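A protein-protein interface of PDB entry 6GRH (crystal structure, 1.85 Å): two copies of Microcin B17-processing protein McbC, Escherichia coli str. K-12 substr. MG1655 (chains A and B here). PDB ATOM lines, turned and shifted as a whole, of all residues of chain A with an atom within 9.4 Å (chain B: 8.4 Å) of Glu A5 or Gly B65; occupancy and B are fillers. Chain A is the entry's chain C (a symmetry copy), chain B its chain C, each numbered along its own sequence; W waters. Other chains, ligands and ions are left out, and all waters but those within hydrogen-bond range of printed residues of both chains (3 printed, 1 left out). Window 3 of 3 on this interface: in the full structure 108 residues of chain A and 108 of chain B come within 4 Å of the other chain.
No position is printed for both chains.
The side-chain carboxylate of Glu B59 sits at hydrogen-bond distance from the backbone NH of Ser A2, at 2.9 Å. N of Glu B59 sits at hydrogen-bond distance from O of His A4 (2.8 Å). O of Glu B59 is in hydrogen-bond range of N of Leu A6, 2.9 Å away. OE2 of Glu B59 is in hydrogen-bond range of N of Leu A155, at 2.8 Å. The side-chain carboxylate (OE1) of Glu B59 is in hydrogen-bond range of the side-chain hydroxyl (OG) of Ser A156, 2.6 Å away. The side-chain carboxylate of Glu A160 sits at hydrogen-bond distance from the backbone NH of Phe B62 (2.9 Å). The backbone NH (N) of Arg B63 sits at hydrogen-bond distance from the side-chain carboxylate (OE2) of Glu A160. N of Gly B65 sits at hydrogen-bond distance from OE2 of Glu A5. The side-chain carboxylate of Glu B59 sits close to the backbone carbonyl oxygen of Leu A153, at 3.4 Å.
Of the printed residues of chain B, His A4 touches Lys B58 and Glu B59. Glu A5 touches four residues of chain B. Printed residues of chain B within 4 Å of Leu A153: Glu B59 and Leu B61. Of the printed residues of chain B, Ser A156 touches Glu B59 (2.6 Å). Of the printed residues of chain A, Leu B61 touches Glu A5, Leu A153 and Glu A160. Of the printed residues of chain A, Phe B62 touches His A151 (3.8 Å) and Glu A160 (2.9 Å). Of the printed residues of chain A, Pro B64 touches Glu A5. Gly B65 touches just one residue of chain A: Glu A5. Ser B68 touches none of the printed residues of chain A. The nearest residue of chain B that does not touch Glu A5 is Lys B58 (4.2 Å). The nearest printed residue of chain A that does not touch Phe B62 is Leu A153 (5.7 Å).
Water W2 lies within hydrogen-bond range of the backbone carbonyl oxygen of Val A116 (2.7 Å) and the side-chain amide oxygen of Asn B57 (2.7 Å). Water W3 lies within hydrogen-bond range of the side-chain carboxylate of Glu A5, the backbone carbonyl oxygen of Phe B66 and the backbone NH of Gly B65. Water W1 bridges O of Leu A6 (2.8 Å) and N of Leu B61 (3.0 Å).
The backbone carbonyl oxygen of Glu B56 is in hydrogen-bond range of the side-chain amino group of Lys B58, 2.9 Å away. The backbone NH (N) of Ser A2 is in hydrogen-bond range of the side-chain hydroxyl (OG) of Ser A156, at 3.4 Å. OE1 of Glu A160 sits at hydrogen-bond distance from ND1 of His A151, at 2.8 Å.
Among the printed residues, 28 pairs touch across the chains. Among the printed residues, no Asp or Glu carboxylate lies within 4 Å of a Lys or Arg side-chain nitrogen of the other chain.
Glu B59 touches Glu A5 (O to CA, 3.4 Å). Leu B61 touches Glu A5. CA of Pro B64 touches OE2 of Glu A5 (3.5 Å). Leu A6 touches Phe B55 (CD1 to CD1, 3.9 Å). CG1 of Val B60 touches CD1 of Leu A8 (3.7 Å). CZ of Phe B55 touches O of Glu A10, at 3.6 Å. Val B60 touches His A151. Phe B62 touches His A151. Leu A155 touches Asn B57 (CD1 to O, 3.2 Å). CB of Leu B61 touches OE2 of Glu A160, 3.6 Å away.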
ATOM      1  N   SER A   2     -24.321  -8.726 -25.597  1.00  0.00           N
ATOM      2  CA  SER A   2     -22.833  -8.626 -25.350  1.00  0.00           C
ATOM      3  C   SER A   2     -22.435  -7.237 -24.798  1.00  0.00           C
ATOM      4  O   SER A   2     -21.927  -7.145 -23.674  1.00  0.00           O
ATOM      5  CB  SER A   2     -22.050  -8.971 -26.614  1.00  0.00           C
ATOM      6  N   LYS A   3     -22.674  -6.171 -25.571  1.00  0.00           N
ATOM      7  CA  LYS A   3     -22.802  -4.808 -25.006  1.00  0.00           C
ATOM      8  C   LYS A   3     -24.043  -4.708 -24.075  1.00  0.00           C
ATOM      9  O   LYS A   3     -24.117  -3.839 -23.216  1.00  0.00           O
ATOM     10  CB  LYS A   3     -22.935  -3.763 -26.116  1.00  0.00           C
ATOM     11  N   HIS A   4     -25.013  -5.590 -24.296  1.00  0.00           N
ATOM     12  CA  HIS A   4     -26.269  -5.633 -23.562  1.00  0.00           C
ATOM     13  C   HIS A   4     -26.340  -6.787 -22.534  1.00  0.00           C
ATOM     14  O   HIS A   4     -27.433  -7.197 -22.131  1.00  0.00           O
ATOM     15  CB  HIS A   4     -27.404  -5.788 -24.581  1.00  0.00           C
ATOM     16  CG  HIS A   4     -27.321  -4.828 -25.729  1.00  0.00           C
ATOM     17  ND1 HIS A   4     -27.652  -3.497 -25.608  1.00  0.00           N
ATOM     18  CD2 HIS A   4     -26.922  -5.005 -27.013  1.00  0.00           C
ATOM     19  CE1 HIS A   4     -27.461  -2.890 -26.767  1.00  0.00           C
ATOM     20  NE2 HIS A   4     -27.020  -3.784 -27.639  1.00  0.00           N
ATOM     21  N   GLU A   5     -25.187  -7.289 -22.102  1.00  0.00           N
ATOM     22  CA  GLU A   5     -25.142  -8.510 -21.313  1.00  0.00           C
ATOM     23  C   GLU A   5     -25.701  -8.284 -19.915  1.00  0.00           C
ATOM     24  O   GLU A   5     -25.475  -7.256 -19.317  1.00  0.00           O
ATOM     25  CB  GLU A   5     -23.708  -9.057 -21.213  1.00  0.00           C
ATOM     26  CG  GLU A   5     -23.638 -10.498 -20.696  1.00  0.00           C
ATOM     27  CD  GLU A   5     -22.210 -11.004 -20.499  1.00  0.00           C
ATOM     28  OE1 GLU A   5     -21.260 -10.333 -20.943  1.00  0.00           O
ATOM     29  OE2 GLU A   5     -22.053 -12.082 -19.886  1.00  0.00           O
ATOM     30  N   LEU A   6     -26.476  -9.246 -19.438  1.00  0.00           N
ATOM     31  CA  LEU A   6     -26.937  -9.299 -18.070  1.00  0.00           C
ATOM     32  C   LEU A   6     -26.484 -10.646 -17.519  1.00  0.00           C
ATOM     33  O   LEU A   6     -26.737 -11.694 -18.136  1.00  0.00           O
ATOM     34  CB  LEU A   6     -28.466  -9.238 -18.025  1.00  0.00           C
ATOM     35  CG  LEU A   6     -29.131  -9.616 -16.690  1.00  0.00           C
ATOM     36  CD1 LEU A   6     -28.673  -8.651 -15.604  1.00  0.00           C
ATOM     37  CD2 LEU A   6     -30.637  -9.619 -16.851  1.00  0.00           C
ATOM     38  N   SER A   7     -25.856 -10.617 -16.353  1.00  0.00           N
ATOM     39  CA  SER A   7     -25.475 -11.836 -15.667  1.00  0.00           C
ATOM     40  C   SER A   7     -26.658 -12.353 -14.851  1.00  0.00           C
ATOM     41  O   SER A   7     -27.265 -11.597 -14.098  1.00  0.00           O
ATOM     42  CB  SER A   7     -24.299 -11.581 -14.725  1.00  0.00           C
ATOM     43  OG  SER A   7     -24.018 -12.781 -14.010  1.00  0.00           O
ATOM     44  N   LEU A   8     -26.939 -13.649 -14.949  1.00  0.00           N
ATOM     45  CA  LEU A   8     -27.966 -14.257 -14.102  1.00  0.00           C
ATOM     46  C   LEU A   8     -27.670 -14.207 -12.567  1.00  0.00           C
ATOM     47  O   LEU A   8     -28.591 -14.358 -11.760  1.00  0.00           O
ATOM     48  CB  LEU A   8     -28.258 -15.688 -14.582  1.00  0.00           C
ATOM     49  CG  LEU A   8     -28.929 -15.762 -15.951  1.00  0.00           C
ATOM     50  CD1 LEU A   8     -29.037 -17.201 -16.452  1.00  0.00           C
ATOM     51  CD2 LEU A   8     -30.297 -15.089 -15.907  1.00  0.00           C
ATOM     52  N   VAL A   9     -26.405 -14.005 -12.203  1.00  0.00           N
ATOM     53  CA  VAL A   9     -26.002 -13.740 -10.823  1.00  0.00           C
ATOM     54  C   VAL A   9     -26.787 -12.575 -10.225  1.00  0.00           C
ATOM     55  O   VAL A   9     -27.219 -12.637  -9.077  1.00  0.00           O
ATOM     56  CB  VAL A   9     -24.501 -13.429 -10.745  1.00  0.00           C
ATOM     57  CG1 VAL A   9     -24.099 -13.078  -9.312  1.00  0.00           C
ATOM     58  CG2 VAL A   9     -23.692 -14.614 -11.278  1.00  0.00           C
ATOM     59  N   GLU A  10     -26.987 -11.536 -11.034  1.00  0.00           N
ATOM     60  CA  GLU A  10     -27.697 -10.319 -10.609  1.00  0.00           C
ATOM     61  C   GLU A  10     -29.182 -10.616 -10.386  1.00  0.00           C
ATOM     62  O   GLU A  10     -29.788 -10.079  -9.460  1.00  0.00           O
ATOM     63  CB  GLU A  10     -27.540  -9.182 -11.638  1.00  0.00           C
ATOM     64  CG  GLU A  10     -26.109  -8.716 -11.871  1.00  0.00           C
ATOM     65  CD  GLU A  10     -25.571  -7.769 -10.802  1.00  0.00           C
ATOM     66  OE1 GLU A  10     -26.288  -7.471  -9.813  1.00  0.00           O
ATOM     67  OE2 GLU A  10     -24.411  -7.280 -10.968  1.00  0.00           O
ATOM     68  N   VAL A  11     -29.735 -11.466 -11.243  1.00  0.00           N
ATOM     69  CA  VAL A  11     -31.119 -11.887 -11.159  1.00  0.00           C
ATOM     70  C   VAL A  11     -31.375 -12.717  -9.909  1.00  0.00           C
ATOM     71  O   VAL A  11     -32.335 -12.441  -9.171  1.00  0.00           O
ATOM     72  CB  VAL A  11     -31.555 -12.648 -12.438  1.00  0.00           C
ATOM     73  CG1 VAL A  11     -32.920 -13.293 -12.271  1.00  0.00           C
ATOM     74  CG2 VAL A  11     -31.539 -11.680 -13.598  1.00  0.00           C
ATOM     75  N   VAL A 116     -32.509  -0.758 -28.634  1.00  0.00           N
ATOM     76  CA  VAL A 116     -32.826  -1.912 -27.787  1.00  0.00           C
ATOM     77  C   VAL A 116     -34.319  -2.287 -27.709  1.00  0.00           C
ATOM     78  O   VAL A 116     -34.685  -3.184 -26.919  1.00  0.00           O
ATOM     79  CB  VAL A 116     -32.264  -1.736 -26.361  1.00  0.00           C
ATOM     80  CG1 VAL A 116     -30.771  -1.418 -26.432  1.00  0.00           C
ATOM     81  CG2 VAL A 116     -33.050  -0.674 -25.571  1.00  0.00           C
ATOM     82  N   HIS A 151     -27.790 -19.731 -30.390  1.00  0.00           N
ATOM     83  CA  HIS A 151     -28.667 -18.907 -29.595  1.00  0.00           C
ATOM     84  C   HIS A 151     -28.720 -17.533 -30.267  1.00  0.00           C
ATOM     85  O   HIS A 151     -27.680 -16.943 -30.508  1.00  0.00           O
ATOM     86  CB  HIS A 151     -28.101 -18.869 -28.186  1.00  0.00           C
ATOM     87  CG  HIS A 151     -28.746 -17.882 -27.274  1.00  0.00           C
ATOM     88  ND1 HIS A 151     -28.015 -17.075 -26.436  1.00  0.00           N
ATOM     89  CD2 HIS A 151     -30.044 -17.582 -27.053  1.00  0.00           C
ATOM     90  CE1 HIS A 151     -28.836 -16.315 -25.728  1.00  0.00           C
ATOM     91  NE2 HIS A 151     -30.076 -16.614 -26.074  1.00  0.00           N
ATOM     92  N   LEU A 153     -29.191 -13.639 -30.332  1.00  0.00           N
ATOM     93  CA  LEU A 153     -29.100 -12.471 -29.451  1.00  0.00           C
ATOM     94  C   LEU A 153     -29.821 -11.335 -30.161  1.00  0.00           C
ATOM     95  O   LEU A 153     -29.267 -10.738 -31.093  1.00  0.00           O
ATOM     96  CB  LEU A 153     -27.638 -12.119 -29.152  1.00  0.00           C
ATOM     97  CG  LEU A 153     -26.764 -13.201 -28.513  1.00  0.00           C
ATOM     98  CD1 LEU A 153     -25.314 -12.744 -28.431  1.00  0.00           C
ATOM     99  CD2 LEU A 153     -27.281 -13.575 -27.122  1.00  0.00           C
ATOM    100  N   LEU A 155     -30.706  -8.187 -29.511  1.00  0.00           N
ATOM    101  CA  LEU A 155     -30.237  -6.810 -29.426  1.00  0.00           C
ATOM    102  C   LEU A 155     -28.903  -6.668 -30.140  1.00  0.00           C
ATOM    103  O   LEU A 155     -28.728  -5.725 -30.880  1.00  0.00           O
ATOM    104  CB  LEU A 155     -30.149  -6.351 -27.966  1.00  0.00           C
ATOM    105  CG  LEU A 155     -31.480  -6.439 -27.211  1.00  0.00           C
ATOM    106  CD1 LEU A 155     -31.349  -5.862 -25.805  1.00  0.00           C
ATOM    107  CD2 LEU A 155     -32.578  -5.730 -27.983  1.00  0.00           C
ATOM    108  N   SER A 156     -27.990  -7.628 -29.946  1.00  0.00           N
ATOM    109  CA  SER A 156     -26.724  -7.654 -30.697  1.00  0.00           C
ATOM    110  C   SER A 156     -26.943  -8.003 -32.188  1.00  0.00           C
ATOM    111  O   SER A 156     -26.126  -7.645 -33.039  1.00  0.00           O
ATOM    112  CB  SER A 156     -25.750  -8.675 -30.102  1.00  0.00           C
ATOM    113  OG  SER A 156     -25.464  -8.427 -28.746  1.00  0.00           O
ATOM    114  N   GLU A 160     -24.938 -16.904 -31.283  1.00  0.00           N
ATOM    115  CA  GLU A 160     -23.943 -17.489 -30.401  1.00  0.00           C
ATOM    116  C   GLU A 160     -23.929 -19.027 -30.602  1.00  0.00           C
ATOM    117  O   GLU A 160     -24.985 -19.644 -30.569  1.00  0.00           O
ATOM    118  CB  GLU A 160     -24.365 -17.109 -28.986  1.00  0.00           C
ATOM    119  CG  GLU A 160     -23.439 -17.491 -27.854  1.00  0.00           C
ATOM    120  CD  GLU A 160     -24.004 -17.072 -26.485  1.00  0.00           C
ATOM    121  OE1 GLU A 160     -25.257 -17.041 -26.282  1.00  0.00           O
ATOM    122  OE2 GLU A 160     -23.183 -16.792 -25.591  1.00  0.00           O
ATOM    123  N   LYS A 197     -35.432 -15.420 -14.438  1.00  0.00           N
ATOM    124  CA  LYS A 197     -35.677 -14.151 -15.111  1.00  0.00           C
ATOM    125  C   LYS A 197     -37.179 -13.875 -15.243  1.00  0.00           C
ATOM    126  O   LYS A 197     -37.592 -12.722 -15.157  1.00  0.00           O
ATOM    127  CB  LYS A 197     -35.020 -14.108 -16.475  1.00  0.00           C
ATOM    128  CG  LYS A 197     -35.009 -12.705 -17.059  1.00  0.00           C
ATOM    129  CD  LYS A 197     -33.657 -12.375 -17.623  1.00  0.00           C
ATOM    130  CE  LYS A 197     -33.686 -11.074 -18.394  1.00  0.00           C
ATOM    131  NZ  LYS A 197     -33.641 -11.267 -19.875  1.00  0.00           N
ATOM    132  N   LYS B  54     -30.745  -2.007 -14.682  1.00  0.00           N
ATOM    133  CA  LYS B  54     -29.770  -3.039 -15.018  1.00  0.00           C
ATOM    134  C   LYS B  54     -30.392  -4.334 -15.593  1.00  0.00           C
ATOM    135  O   LYS B  54     -29.691  -5.130 -16.215  1.00  0.00           O
ATOM    136  CB  LYS B  54     -28.837  -3.339 -13.824  1.00  0.00           C
ATOM    137  CG  LYS B  54     -29.161  -4.581 -12.991  1.00  0.00           C
ATOM    138  CD  LYS B  54     -27.960  -5.044 -12.158  1.00  0.00           C
ATOM    139  CE  LYS B  54     -27.634  -4.120 -11.001  1.00  0.00           C
ATOM    140  NZ  LYS B  54     -28.709  -4.163  -9.965  1.00  0.00           N
ATOM    141  N   PHE B  55     -31.690  -4.541 -15.381  1.00  0.00           N
ATOM    142  CA  PHE B  55     -32.387  -5.724 -15.858  1.00  0.00           C
ATOM    143  C   PHE B  55     -33.196  -5.546 -17.144  1.00  0.00           C
ATOM    144  O   PHE B  55     -33.565  -6.531 -17.780  1.00  0.00           O
ATOM    145  CB  PHE B  55     -33.298  -6.243 -14.764  1.00  0.00           C
ATOM    146  CG  PHE B  55     -32.567  -6.603 -13.519  1.00  0.00           C
ATOM    147  CD1 PHE B  55     -31.820  -7.792 -13.452  1.00  0.00           C
ATOM    148  CD2 PHE B  55     -32.597  -5.772 -12.410  1.00  0.00           C
ATOM    149  CE1 PHE B  55     -31.145  -8.137 -12.294  1.00  0.00           C
ATOM    150  CE2 PHE B  55     -31.929  -6.133 -11.239  1.00  0.00           C
ATOM    151  CZ  PHE B  55     -31.194  -7.300 -11.188  1.00  0.00           C
ATOM    152  N   GLU B  56     -33.460  -4.299 -17.515  1.00  0.00           N
ATOM    153  CA  GLU B  56     -34.358  -3.983 -18.601  1.00  0.00           C
ATOM    154  C   GLU B  56     -33.588  -3.996 -19.936  1.00  0.00           C
ATOM    155  O   GLU B  56     -32.491  -3.430 -20.042  1.00  0.00           O
ATOM    156  CB  GLU B  56     -35.015  -2.619 -18.342  1.00  0.00           C
ATOM    157  CG  GLU B  56     -35.988  -2.665 -17.164  1.00  0.00           C
ATOM    158  CD  GLU B  56     -36.436  -1.296 -16.656  1.00  0.00           C
ATOM    159  OE1 GLU B  56     -35.899  -0.251 -17.069  1.00  0.00           O
ATOM    160  OE2 GLU B  56     -37.316  -1.265 -15.799  1.00  0.00           O
ATOM    161  N   ASN B  57     -34.173  -4.671 -20.928  1.00  0.00           N
ATOM    162  CA  ASN B  57     -33.663  -4.693 -22.305  1.00  0.00           C
ATOM    163  C   ASN B  57     -32.231  -5.192 -22.388  1.00  0.00           C
ATOM    164  O   ASN B  57     -31.361  -4.519 -22.935  1.00  0.00           O
ATOM    165  CB  ASN B  57     -33.777  -3.307 -22.966  1.00  0.00           C
ATOM    166  CG  ASN B  57     -35.210  -2.827 -23.036  1.00  0.00           C
ATOM    167  OD1 ASN B  57     -36.086  -3.523 -23.548  1.00  0.00           O
ATOM    168  ND2 ASN B  57     -35.453  -1.652 -22.519  1.00  0.00           N
ATOM    169  N   LYS B  58     -32.010  -6.374 -21.829  1.00  0.00           N
ATOM    170  CA  LYS B  58     -30.701  -7.003 -21.793  1.00  0.00           C
ATOM    171  C   LYS B  58     -30.745  -8.366 -22.487  1.00  0.00           C
ATOM    172  O   LYS B  58     -31.810  -8.855 -22.829  1.00  0.00           O
ATOM    173  CB  LYS B  58     -30.256  -7.158 -20.344  1.00  0.00           C
ATOM    174  CG  LYS B  58     -30.035  -5.835 -19.588  1.00  0.00           C
ATOM    175  CD  LYS B  58     -28.885  -5.018 -20.140  1.00  0.00           C
ATOM    176  CE  LYS B  58     -28.607  -3.776 -19.311  1.00  0.00           C
ATOM    177  NZ  LYS B  58     -29.792  -2.877 -19.289  1.00  0.00           N
ATOM    178  N   GLU B  59     -29.572  -8.943 -22.705  1.00  0.00           N
ATOM    179  CA  GLU B  59     -29.413 -10.299 -23.243  1.00  0.00           C
ATOM    180  C   GLU B  59     -28.684 -11.140 -22.217  1.00  0.00           C
ATOM    181  O   GLU B  59     -27.653 -10.730 -21.678  1.00  0.00           O
ATOM    182  CB  GLU B  59     -28.572 -10.298 -24.516  1.00  0.00           C
ATOM    183  CG  GLU B  59     -29.112  -9.399 -25.599  1.00  0.00           C
ATOM    184  CD  GLU B  59     -28.231  -9.314 -26.839  1.00  0.00           C
ATOM    185  OE1 GLU B  59     -26.989  -9.068 -26.753  1.00  0.00           O
ATOM    186  OE2 GLU B  59     -28.834  -9.463 -27.921  1.00  0.00           O
ATOM    187  N   VAL B  60     -29.217 -12.324 -21.955  1.00  0.00           N
ATOM    188  CA  VAL B  60     -28.498 -13.321 -21.192  1.00  0.00           C
ATOM    189  C   VAL B  60     -27.770 -14.177 -22.228  1.00  0.00           C
ATOM    190  O   VAL B  60     -28.325 -14.478 -23.286  1.00  0.00           O
ATOM    191  CB  VAL B  60     -29.463 -14.161 -20.338  1.00  0.00           C
ATOM    192  CG1 VAL B  60     -28.727 -15.307 -19.657  1.00  0.00           C
ATOM    193  CG2 VAL B  60     -30.147 -13.263 -19.321  1.00  0.00           C
ATOM    194  N   LEU B  61     -26.539 -14.556 -21.922  1.00  0.00           N
ATOM    195  CA  LEU B  61     -25.710 -15.344 -22.841  1.00  0.00           C
ATOM    196  C   LEU B  61     -25.630 -16.834 -22.483  1.00  0.00           C
ATOM    197  O   LEU B  61     -25.598 -17.217 -21.301  1.00  0.00           O
ATOM    198  CB  LEU B  61     -24.303 -14.751 -22.875  1.00  0.00           C
ATOM    199  CG  LEU B  61     -24.160 -13.310 -23.364  1.00  0.00           C
ATOM    200  CD1 LEU B  61     -22.689 -12.993 -23.557  1.00  0.00           C
ATOM    201  CD2 LEU B  61     -24.930 -13.090 -24.657  1.00  0.00           C
ATOM    202  N   PHE B  62     -25.589 -17.674 -23.520  1.00  0.00           N
ATOM    203  CA  PHE B  62     -25.217 -19.083 -23.362  1.00  0.00           C
ATOM    204  C   PHE B  62     -23.764 -19.254 -22.890  1.00  0.00           C
ATOM    205  O   PHE B  62     -23.513 -20.144 -22.085  1.00  0.00           O
ATOM    206  CB  PHE B  62     -25.466 -19.887 -24.636  1.00  0.00           C
ATOM    207  CG  PHE B  62     -25.380 -21.366 -24.431  1.00  0.00           C
ATOM    208  CD1 PHE B  62     -26.451 -22.069 -23.897  1.00  0.00           C
ATOM    209  CD2 PHE B  62     -24.234 -22.052 -24.762  1.00  0.00           C
ATOM    210  CE1 PHE B  62     -26.384 -23.445 -23.704  1.00  0.00           C
ATOM    211  CE2 PHE B  62     -24.156 -23.430 -24.577  1.00  0.00           C
ATOM    212  CZ  PHE B  62     -25.238 -24.116 -24.048  1.00  0.00           C
ATOM    213  N   ARG B  63     -22.840 -18.390 -23.322  1.00  0.00           N
ATOM    214  CA  ARG B  63     -21.441 -18.376 -22.788  1.00  0.00           C
ATOM    215  C   ARG B  63     -21.083 -16.999 -22.193  1.00  0.00           C
ATOM    216  O   ARG B  63     -20.422 -16.192 -22.850  1.00  0.00           O
ATOM    217  CB  ARG B  63     -20.411 -18.831 -23.845  1.00  0.00           C
ATOM    218  CG  ARG B  63     -20.508 -20.330 -24.125  1.00  0.00           C
ATOM    219  CD  ARG B  63     -19.355 -20.907 -24.936  1.00  0.00           C
ATOM    220  NE  ARG B  63     -19.527 -22.365 -25.052  1.00  0.00           N
ATOM    221  CZ  ARG B  63     -20.297 -22.998 -25.948  1.00  0.00           C
ATOM    222  NH1 ARG B  63     -20.988 -22.338 -26.873  1.00  0.00           N
ATOM    223  NH2 ARG B  63     -20.377 -24.322 -25.926  1.00  0.00           N
ATOM    224  N   PRO B  64     -21.548 -16.732 -20.946  1.00  0.00           N
ATOM    225  CA  PRO B  64     -21.278 -15.455 -20.264  1.00  0.00           C
ATOM    226  C   PRO B  64     -19.807 -15.187 -20.183  1.00  0.00           C
ATOM    227  O   PRO B  64     -19.027 -16.111 -19.933  1.00  0.00           O
ATOM    228  CB  PRO B  64     -21.831 -15.663 -18.842  1.00  0.00           C
ATOM    229  CG  PRO B  64     -22.664 -16.866 -18.885  1.00  0.00           C
ATOM    230  CD  PRO B  64     -22.258 -17.683 -20.070  1.00  0.00           C
ATOM    231  N   GLY B  65     -19.416 -13.937 -20.406  1.00  0.00           N
ATOM    232  CA  GLY B  65     -18.004 -13.569 -20.396  1.00  0.00           C
ATOM    233  C   GLY B  65     -17.303 -13.703 -21.729  1.00  0.00           C
ATOM    234  O   GLY B  65     -16.175 -13.243 -21.866  1.00  0.00           O
ATOM    235  N   PHE B  66     -17.956 -14.316 -22.717  1.00  0.00           N
ATOM    236  CA  PHE B  66     -17.346 -14.537 -24.036  1.00  0.00           C
ATOM    237  C   PHE B  66     -18.133 -13.833 -25.118  1.00  0.00           C
ATOM    238  O   PHE B  66     -19.307 -13.625 -24.984  1.00  0.00           O
ATOM    239  CB  PHE B  66     -17.172 -16.044 -24.286  1.00  0.00           C
ATOM    240  CG  PHE B  66     -16.310 -16.684 -23.248  1.00  0.00           C
ATOM    241  CD1 PHE B  66     -14.951 -16.514 -23.292  1.00  0.00           C
ATOM    242  CD2 PHE B  66     -16.870 -17.345 -22.163  1.00  0.00           C
ATOM    243  CE1 PHE B  66     -14.136 -17.040 -22.308  1.00  0.00           C
ATOM    244  CE2 PHE B  66     -16.060 -17.879 -21.174  1.00  0.00           C
ATOM    245  CZ  PHE B  66     -14.695 -17.722 -21.248  1.00  0.00           C
ATOM    246  N   SER B  67     -17.438 -13.425 -26.168  1.00  0.00           N
ATOM    247  CA  SER B  67     -17.968 -12.493 -27.167  1.00  0.00           C
ATOM    248  C   SER B  67     -17.836 -12.980 -28.621  1.00  0.00           C
ATOM    249  O   SER B  67     -18.074 -12.203 -29.543  1.00  0.00           O
ATOM    250  CB  SER B  67     -17.221 -11.168 -27.027  1.00  0.00           C
ATOM    251  OG  SER B  67     -15.844 -11.345 -27.290  1.00  0.00           O
ATOM    252  N   SER B  68     -17.464 -14.248 -28.827  1.00  0.00           N
ATOM    253  CA  SER B  68     -17.347 -14.810 -30.175  1.00  0.00           C
ATOM    254  C   SER B  68     -18.723 -15.134 -30.691  1.00  0.00           C
ATOM    255  O   SER B  68     -19.352 -16.077 -30.241  1.00  0.00           O
ATOM    256  CB  SER B  68     -16.494 -16.070 -30.169  1.00  0.00           C
ATOM    257  OG  SER B  68     -15.186 -15.710 -29.807  1.00  0.00           O
HETATM  258  O   HOH W   1     -25.254 -13.762 -19.294  1.00  0.00           O
HETATM  259  O   HOH W   2     -34.979  -5.289 -25.332  1.00  0.00           O
HETATM  260  O   HOH W   3     -19.410 -11.423 -22.613  1.00  0.00           O
